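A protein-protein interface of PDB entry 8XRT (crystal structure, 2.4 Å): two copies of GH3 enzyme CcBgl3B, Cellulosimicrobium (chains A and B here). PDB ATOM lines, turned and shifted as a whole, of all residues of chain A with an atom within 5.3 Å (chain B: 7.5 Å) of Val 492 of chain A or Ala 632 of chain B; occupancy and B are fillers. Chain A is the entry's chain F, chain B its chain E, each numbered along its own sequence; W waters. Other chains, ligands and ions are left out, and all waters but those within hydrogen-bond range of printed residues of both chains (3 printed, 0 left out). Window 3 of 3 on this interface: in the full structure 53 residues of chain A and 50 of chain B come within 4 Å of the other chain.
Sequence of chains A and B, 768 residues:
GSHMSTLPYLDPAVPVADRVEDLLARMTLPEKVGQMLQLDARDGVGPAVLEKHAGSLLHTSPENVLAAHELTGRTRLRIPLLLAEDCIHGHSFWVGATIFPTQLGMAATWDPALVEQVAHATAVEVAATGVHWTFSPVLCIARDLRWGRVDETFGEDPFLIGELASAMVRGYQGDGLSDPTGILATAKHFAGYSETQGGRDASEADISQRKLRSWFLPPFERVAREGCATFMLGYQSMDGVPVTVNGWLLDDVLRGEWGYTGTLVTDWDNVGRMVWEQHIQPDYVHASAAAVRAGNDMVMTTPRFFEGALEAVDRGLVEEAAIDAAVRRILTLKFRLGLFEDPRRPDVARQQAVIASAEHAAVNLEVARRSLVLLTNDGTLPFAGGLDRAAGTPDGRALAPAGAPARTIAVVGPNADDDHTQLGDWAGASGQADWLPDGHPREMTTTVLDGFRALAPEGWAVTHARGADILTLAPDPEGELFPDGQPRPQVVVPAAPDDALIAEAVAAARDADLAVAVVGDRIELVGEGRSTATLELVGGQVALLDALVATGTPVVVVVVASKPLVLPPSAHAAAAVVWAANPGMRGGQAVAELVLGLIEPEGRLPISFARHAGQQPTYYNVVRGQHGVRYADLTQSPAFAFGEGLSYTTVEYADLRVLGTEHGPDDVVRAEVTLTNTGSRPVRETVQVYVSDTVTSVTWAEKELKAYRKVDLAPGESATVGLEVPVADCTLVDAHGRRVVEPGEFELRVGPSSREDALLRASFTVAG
Of the 15 printed residues of chain A, 6 touch a printed residue of chain B. Hydrophobic or aromatic side chains of chain A within 4 Å of the printed part of chain B: Val 491, Val 492 and Leu 525. Of the 7 printed residues of chain B, 4 touch a printed residue of chain A. Printed residues of chain B that touch a printed residue of chain A: Arg 630, Tyr 631, Ala 632 and Asp 633. Among the printed residues, 8 pairs touch across the chains. Among the printed residues, no Asp or Glu carboxylate lies within 4 Å of a Lys or Arg side-chain nitrogen of the other chain.
No position is printed for both chains.
CG2 of Val 491 of chain A touches CD of Arg 630 of chain B (3.9 Å). CB of Val 492 of chain A touches O of Ala 632 of chain B, 3.5 Å away. Ala 632 of chain B touches Glu 524 of chain A. Ala 632 of chain B touches Leu 525 of chain A (CB to CD2, 3.9 Å). Ser 531 of chain A touches Tyr 631 of chain B. Tyr 631 of chain B touches Thr 532 of chain A (CD1 to C, 3.5 Å). OD1 of Asp 633 of chain B touches CA of Thr 532 of chain A, 3.4 Å away.
Water W2 lies within hydrogen-bond range of the backbone carbonyl oxygen (O) of Val 492 of chain A (2.8 Å), the guanidinium group (NH2) of Arg 630 of chain B (3.0 Å) and the backbone carbonyl oxygen (O) of Ala 632 of chain B (3.0 Å). Water W3 lies within hydrogen-bond range of the backbone carbonyl oxygen (O) of Arg 630 of chain B (2.9 Å) and the backbone NH (N) of Ser 531 of chain A (3.0 Å). Water W1 lies within hydrogen-bond range of O of Ala 632 of chain B, N of Val 492 of chain A and NE of Arg 630 of chain B.
The backbone carbonyl oxygen (O) of Ala 474 of chain A lies within hydrogen-bond range of the backbone NH (N) of Val 491 of chain A (2.9 Å).
The backbone NH (N) of Ala 632 of chain B lies within hydrogen-bond range of the backbone carbonyl oxygen (O) of Ser 531 of chain A (2.7 Å).
Of the printed residues of chain B, Val 491 of chain A touches Arg 630 (3.9 Å). Of chain B, only Ala 632 comes within 4 Å of Val 492 of chain A. Of the printed residues of chain B, Glu 524 of chain A touches Ala 632. Of the printed residues of chain B, Leu 525 of chain A touches Ala 632. Of chain A, only Val 492, Glu 524, Leu 525 and Ser 531 come within 4 Å of Ala 632 of chain B. The nearest residue of chain A that does not touch Ala 632 of chain B is Arg 530 of chain A (4.2 Å). The nearest printed residue of chain B that does not touch Glu 524 of chain A is Asp 633 of chain B (6.3 Å).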
ATOM      1  N   LEU A 471     -10.583  -9.185  25.933  1.00  0.00           N
ATOM      2  CA  LEU A 471     -10.964  -9.369  24.535  1.00  0.00           C
ATOM      3  C   LEU A 471     -12.468  -9.180  24.342  1.00  0.00           C
ATOM      4  O   LEU A 471     -13.260  -9.356  25.271  1.00  0.00           O
ATOM      5  CB  LEU A 471     -10.557 -10.759  24.027  1.00  0.00           C
ATOM      6  CG  LEU A 471     -11.172 -12.018  24.678  1.00  0.00           C
ATOM      7  CD1 LEU A 471     -12.449 -12.480  23.975  1.00  0.00           C
ATOM      8  CD2 LEU A 471     -10.142 -13.147  24.689  1.00  0.00           C
ATOM      9  N   THR A 472     -12.840  -8.812  23.107  1.00  0.00           N
ATOM     10  CA  THR A 472     -14.175  -9.006  22.530  1.00  0.00           C
ATOM     11  C   THR A 472     -14.065  -9.911  21.298  1.00  0.00           C
ATOM     12  O   THR A 472     -12.973 -10.176  20.784  1.00  0.00           O
ATOM     13  CB  THR A 472     -14.854  -7.671  22.128  1.00  0.00           C
ATOM     14  OG1 THR A 472     -14.156  -7.058  21.027  1.00  0.00           O
ATOM     15  CG2 THR A 472     -14.950  -6.680  23.304  1.00  0.00           C
ATOM     16  N   LEU A 473     -15.215 -10.392  20.822  1.00  0.00           N
ATOM     17  CA  LEU A 473     -15.303 -11.205  19.616  1.00  0.00           C
ATOM     18  C   LEU A 473     -15.925 -10.402  18.478  1.00  0.00           C
ATOM     19  O   LEU A 473     -16.689  -9.460  18.703  1.00  0.00           O
ATOM     20  CB  LEU A 473     -16.126 -12.477  19.860  1.00  0.00           C
ATOM     21  CG  LEU A 473     -15.541 -13.469  20.884  1.00  0.00           C
ATOM     22  CD1 LEU A 473     -16.563 -14.528  21.319  1.00  0.00           C
ATOM     23  CD2 LEU A 473     -14.253 -14.119  20.377  1.00  0.00           C
ATOM     24  N   ALA A 474     -15.598 -10.784  17.251  1.00  0.00           N
ATOM     25  CA  ALA A 474     -16.066 -10.077  16.068  1.00  0.00           C
ATOM     26  C   ALA A 474     -16.173 -11.069  14.925  1.00  0.00           C
ATOM     27  O   ALA A 474     -15.512 -12.115  14.947  1.00  0.00           O
ATOM     28  CB  ALA A 474     -15.120  -8.930  15.692  1.00  0.00           C
ATOM     29  N   GLN A 490     -16.359 -14.518  15.437  1.00  0.00           N
ATOM     30  CA  GLN A 490     -15.608 -15.765  15.476  1.00  0.00           C
ATOM     31  C   GLN A 490     -14.118 -15.490  15.670  1.00  0.00           C
ATOM     32  O   GLN A 490     -13.350 -16.415  15.877  1.00  0.00           O
ATOM     33  CB  GLN A 490     -15.829 -16.592  14.192  1.00  0.00           C
ATOM     34  CG  GLN A 490     -15.800 -18.110  14.404  1.00  0.00           C
ATOM     35  CD  GLN A 490     -16.116 -18.926  13.142  1.00  0.00           C
ATOM     36  OE1 GLN A 490     -16.995 -18.567  12.349  1.00  0.00           O
ATOM     37  NE2 GLN A 490     -15.390 -20.032  12.958  1.00  0.00           N
ATOM     38  N   VAL A 491     -13.711 -14.222  15.611  1.00  0.00           N
ATOM     39  CA  VAL A 491     -12.305 -13.833  15.701  1.00  0.00           C
ATOM     40  C   VAL A 491     -12.103 -12.968  16.941  1.00  0.00           C
ATOM     41  O   VAL A 491     -12.879 -12.038  17.193  1.00  0.00           O
ATOM     42  CB  VAL A 491     -11.850 -13.102  14.424  1.00  0.00           C
ATOM     43  CG1 VAL A 491     -10.616 -12.266  14.665  1.00  0.00           C
ATOM     44  CG2 VAL A 491     -11.582 -14.113  13.316  1.00  0.00           C
ATOM     45  N   VAL A 492     -11.050 -13.272  17.709  1.00  0.00           N
ATOM     46  CA  VAL A 492     -10.755 -12.514  18.920  1.00  0.00           C
ATOM     47  C   VAL A 492     -10.208 -11.148  18.547  1.00  0.00           C
ATOM     48  O   VAL A 492      -9.250 -11.039  17.767  1.00  0.00           O
ATOM     49  CB  VAL A 492      -9.751 -13.266  19.811  1.00  0.00           C
ATOM     50  CG1 VAL A 492      -9.084 -12.289  20.836  1.00  0.00           C
ATOM     51  CG2 VAL A 492     -10.415 -14.438  20.507  1.00  0.00           C
ATOM     52  N   VAL A 493     -10.794 -10.103  19.126  1.00  0.00           N
ATOM     53  CA  VAL A 493     -10.302  -8.738  19.005  1.00  0.00           C
ATOM     54  C   VAL A 493      -9.768  -8.322  20.373  1.00  0.00           C
ATOM     55  O   VAL A 493     -10.552  -8.166  21.323  1.00  0.00           O
ATOM     56  CB  VAL A 493     -11.392  -7.766  18.533  1.00  0.00           C
ATOM     57  CG1 VAL A 493     -10.790  -6.360  18.337  1.00  0.00           C
ATOM     58  CG2 VAL A 493     -12.026  -8.267  17.266  1.00  0.00           C
ATOM     59  N   PRO A 494      -8.461  -8.126  20.519  1.00  0.00           N
ATOM     60  CA  PRO A 494      -7.915  -7.704  21.815  1.00  0.00           C
ATOM     61  C   PRO A 494      -8.508  -6.370  22.234  1.00  0.00           C
ATOM     62  O   PRO A 494      -8.611  -5.449  21.429  1.00  0.00           O
ATOM     63  CB  PRO A 494      -6.409  -7.593  21.546  1.00  0.00           C
ATOM     64  CG  PRO A 494      -6.161  -8.462  20.341  1.00  0.00           C
ATOM     65  CD  PRO A 494      -7.416  -8.310  19.500  1.00  0.00           C
ATOM     66  N   GLU A 524     -11.404 -18.254  25.008  1.00  0.00           N
ATOM     67  CA  GLU A 524     -11.206 -17.977  23.580  1.00  0.00           C
ATOM     68  C   GLU A 524      -9.741 -17.962  23.168  1.00  0.00           C
ATOM     69  O   GLU A 524      -9.450 -17.912  21.964  1.00  0.00           O
ATOM     70  CB  GLU A 524     -11.820 -16.627  23.207  1.00  0.00           C
ATOM     71  CG  GLU A 524     -13.332 -16.504  23.419  1.00  0.00           C
ATOM     72  CD  GLU A 524     -13.667 -16.102  24.851  1.00  0.00           C
ATOM     73  OE1 GLU A 524     -12.716 -15.984  25.685  1.00  0.00           O
ATOM     74  OE2 GLU A 524     -14.876 -15.934  25.155  1.00  0.00           O
ATOM     75  N   LEU A 525      -8.818 -17.996  24.135  1.00  0.00           N
ATOM     76  CA  LEU A 525      -7.388 -18.043  23.888  1.00  0.00           C
ATOM     77  C   LEU A 525      -6.782 -19.402  24.247  1.00  0.00           C
ATOM     78  O   LEU A 525      -5.563 -19.503  24.446  1.00  0.00           O
ATOM     79  CB  LEU A 525      -6.726 -16.928  24.705  1.00  0.00           C
ATOM     80  CG  LEU A 525      -7.221 -15.552  24.344  1.00  0.00           C
ATOM     81  CD1 LEU A 525      -6.749 -14.530  25.401  1.00  0.00           C
ATOM     82  CD2 LEU A 525      -6.703 -15.223  22.954  1.00  0.00           C
ATOM     83  N   ARG A 530      -7.220 -23.246  19.096  1.00  0.00           N
ATOM     84  CA  ARG A 530      -6.997 -21.937  19.697  1.00  0.00           C
ATOM     85  C   ARG A 530      -5.584 -21.843  20.281  1.00  0.00           C
ATOM     86  O   ARG A 530      -5.362 -21.356  21.413  1.00  0.00           O
ATOM     87  CB  ARG A 530      -8.056 -21.667  20.761  1.00  0.00           C
ATOM     88  CG  ARG A 530      -9.394 -21.773  20.083  1.00  0.00           C
ATOM     89  CD  ARG A 530     -10.666 -21.272  20.770  1.00  0.00           C
ATOM     90  NE  ARG A 530     -11.016 -21.861  22.080  1.00  0.00           N
ATOM     91  CZ  ARG A 530     -11.459 -23.089  22.365  1.00  0.00           C
ATOM     92  NH1 ARG A 530     -11.729 -23.428  23.644  1.00  0.00           N
ATOM     93  NH2 ARG A 530     -11.485 -24.044  21.461  1.00  0.00           N
ATOM     94  N   SER A 531      -4.609 -22.332  19.508  1.00  0.00           N
ATOM     95  CA  SER A 531      -3.200 -22.025  19.704  1.00  0.00           C
ATOM     96  C   SER A 531      -2.966 -20.510  19.779  1.00  0.00           C
ATOM     97  O   SER A 531      -3.750 -19.721  19.224  1.00  0.00           O
ATOM     98  CB  SER A 531      -2.392 -22.614  18.559  1.00  0.00           C
ATOM     99  OG  SER A 531      -2.390 -24.015  18.592  1.00  0.00           O
ATOM    100  N   THR A 532      -1.896 -20.082  20.444  1.00  0.00           N
ATOM    101  CA  THR A 532      -1.515 -18.680  20.446  1.00  0.00           C
ATOM    102  C   THR A 532      -0.105 -18.554  19.905  1.00  0.00           C
ATOM    103  O   THR A 532       0.697 -19.477  20.026  1.00  0.00           O
ATOM    104  CB  THR A 532      -1.546 -18.066  21.826  1.00  0.00           C
ATOM    105  OG1 THR A 532      -0.743 -18.872  22.697  1.00  0.00           O
ATOM    106  CG2 THR A 532      -2.952 -17.950  22.333  1.00  0.00           C
ATOM    107  N   VAL A 538      -3.105 -10.601  26.735  1.00  0.00           N
ATOM    108  CA  VAL A 538      -3.889  -9.926  25.708  1.00  0.00           C
ATOM    109  C   VAL A 538      -4.736  -8.823  26.337  1.00  0.00           C
ATOM    110  O   VAL A 538      -5.213  -8.941  27.476  1.00  0.00           O
ATOM    111  CB  VAL A 538      -4.748 -10.972  24.954  1.00  0.00           C
ATOM    112  CG1 VAL A 538      -5.761 -10.307  24.009  1.00  0.00           C
ATOM    113  CG2 VAL A 538      -3.834 -11.940  24.192  1.00  0.00           C
ATOM    114  N   ARG B 630      -6.226 -19.754  12.213  1.00  0.00           N
ATOM    115  CA  ARG B 630      -5.485 -18.660  12.829  1.00  0.00           C
ATOM    116  C   ARG B 630      -5.109 -19.001  14.259  1.00  0.00           C
ATOM    117  O   ARG B 630      -5.675 -19.926  14.808  1.00  0.00           O
ATOM    118  CB  ARG B 630      -6.368 -17.412  12.826  1.00  0.00           C
ATOM    119  CG  ARG B 630      -7.593 -17.439  13.722  1.00  0.00           C
ATOM    120  CD  ARG B 630      -8.295 -16.102  13.627  1.00  0.00           C
ATOM    121  NE  ARG B 630      -7.563 -14.987  14.207  1.00  0.00           N
ATOM    122  CZ  ARG B 630      -7.143 -13.920  13.539  1.00  0.00           C
ATOM    123  NH1 ARG B 630      -7.368 -13.809  12.243  1.00  0.00           N
ATOM    124  NH2 ARG B 630      -6.493 -12.964  14.170  1.00  0.00           N
ATOM    125  N   TYR B 631      -4.097 -18.323  14.772  1.00  0.00           N
ATOM    126  CA  TYR B 631      -3.796 -18.385  16.202  1.00  0.00           C
ATOM    127  C   TYR B 631      -4.834 -17.463  16.820  1.00  0.00           C
ATOM    128  O   TYR B 631      -5.322 -16.554  16.175  1.00  0.00           O
ATOM    129  CB  TYR B 631      -2.373 -17.914  16.514  1.00  0.00           C
ATOM    130  CG  TYR B 631      -1.214 -18.695  15.956  1.00  0.00           C
ATOM    131  CD1 TYR B 631      -0.673 -19.758  16.649  1.00  0.00           C
ATOM    132  CD2 TYR B 631      -0.609 -18.323  14.769  1.00  0.00           C
ATOM    133  CE1 TYR B 631       0.408 -20.464  16.159  1.00  0.00           C
ATOM    134  CE2 TYR B 631       0.471 -19.019  14.262  1.00  0.00           C
ATOM    135  CZ  TYR B 631       0.982 -20.095  14.959  1.00  0.00           C
ATOM    136  OH  TYR B 631       2.048 -20.780  14.469  1.00  0.00           O
ATOM    137  N   ALA B 632      -5.173 -17.691  18.064  1.00  0.00           N
ATOM    138  CA  ALA B 632      -6.262 -16.922  18.678  1.00  0.00           C
ATOM    139  C   ALA B 632      -5.814 -15.498  18.961  1.00  0.00           C
ATOM    140  O   ALA B 632      -6.655 -14.631  19.048  1.00  0.00           O
ATOM    141  CB  ALA B 632      -6.699 -17.643  19.900  1.00  0.00           C
ATOM    142  N   ASP B 633      -4.511 -15.289  19.045  1.00  0.00           N
ATOM    143  CA  ASP B 633      -4.060 -13.921  19.238  1.00  0.00           C
ATOM    144  C   ASP B 633      -3.470 -13.314  17.968  1.00  0.00           C
ATOM    145  O   ASP B 633      -2.959 -12.189  18.021  1.00  0.00           O
ATOM    146  CB  ASP B 633      -3.040 -13.843  20.405  1.00  0.00           C
ATOM    147  CG  ASP B 633      -1.779 -14.712  20.192  1.00  0.00           C
ATOM    148  OD1 ASP B 633      -1.709 -15.479  19.207  1.00  0.00           O
ATOM    149  OD2 ASP B 633      -0.855 -14.652  21.050  1.00  0.00           O
ATOM    150  N   LEU B 634      -3.526 -14.020  16.833  1.00  0.00           N
ATOM    151  CA  LEU B 634      -2.760 -13.578  15.675  1.00  0.00           C
ATOM    152  C   LEU B 634      -3.140 -14.354  14.418  1.00  0.00           C
ATOM    153  O   LEU B 634      -3.244 -15.586  14.443  1.00  0.00           O
ATOM    154  CB  LEU B 634      -1.251 -13.721  15.941  1.00  0.00           C
ATOM    155  CG  LEU B 634      -0.366 -12.996  14.923  1.00  0.00           C
ATOM    156  CD1 LEU B 634      -0.557 -11.500  15.090  1.00  0.00           C
ATOM    157  CD2 LEU B 634       1.095 -13.369  15.077  1.00  0.00           C
ATOM    158  N   THR B 635      -3.272 -13.625  13.310  1.00  0.00           N
ATOM    159  CA  THR B 635      -3.441 -14.227  11.993  1.00  0.00           C
ATOM    160  C   THR B 635      -2.228 -15.079  11.625  1.00  0.00           C
ATOM    161  O   THR B 635      -1.114 -14.893  12.130  1.00  0.00           O
ATOM    162  CB  THR B 635      -3.655 -13.138  10.918  1.00  0.00           C
ATOM    163  OG1 THR B 635      -3.826 -13.753   9.635  1.00  0.00           O
ATOM    164  CG2 THR B 635      -2.452 -12.204  10.830  1.00  0.00           C
ATOM    165  N   GLN B 636      -2.458 -16.042  10.740  1.00  0.00           N
ATOM    166  CA  GLN B 636      -1.380 -16.834  10.163  1.00  0.00           C
ATOM    167  C   GLN B 636      -0.939 -16.304   8.811  1.00  0.00           C
ATOM    168  O   GLN B 636      -0.044 -16.874   8.194  1.00  0.00           O
ATOM    169  CB  GLN B 636      -1.819 -18.313  10.056  1.00  0.00           C
ATOM    170  CG  GLN B 636      -1.971 -18.948  11.452  1.00  0.00           C
ATOM    171  CD  GLN B 636      -2.332 -20.441  11.482  1.00  0.00           C
ATOM    172  OE1 GLN B 636      -2.615 -20.974  12.548  1.00  0.00           O
ATOM    173  NE2 GLN B 636      -2.285 -21.106  10.349  1.00  0.00           N
HETATM  174  O   HOH W   1      -8.852 -15.273  17.111  1.00  0.00           O
HETATM  175  O   HOH W   2      -6.859 -12.352  17.083  1.00  0.00           O
HETATM  176  O   HOH W   3      -4.908 -22.083  16.528  1.00  0.00           O
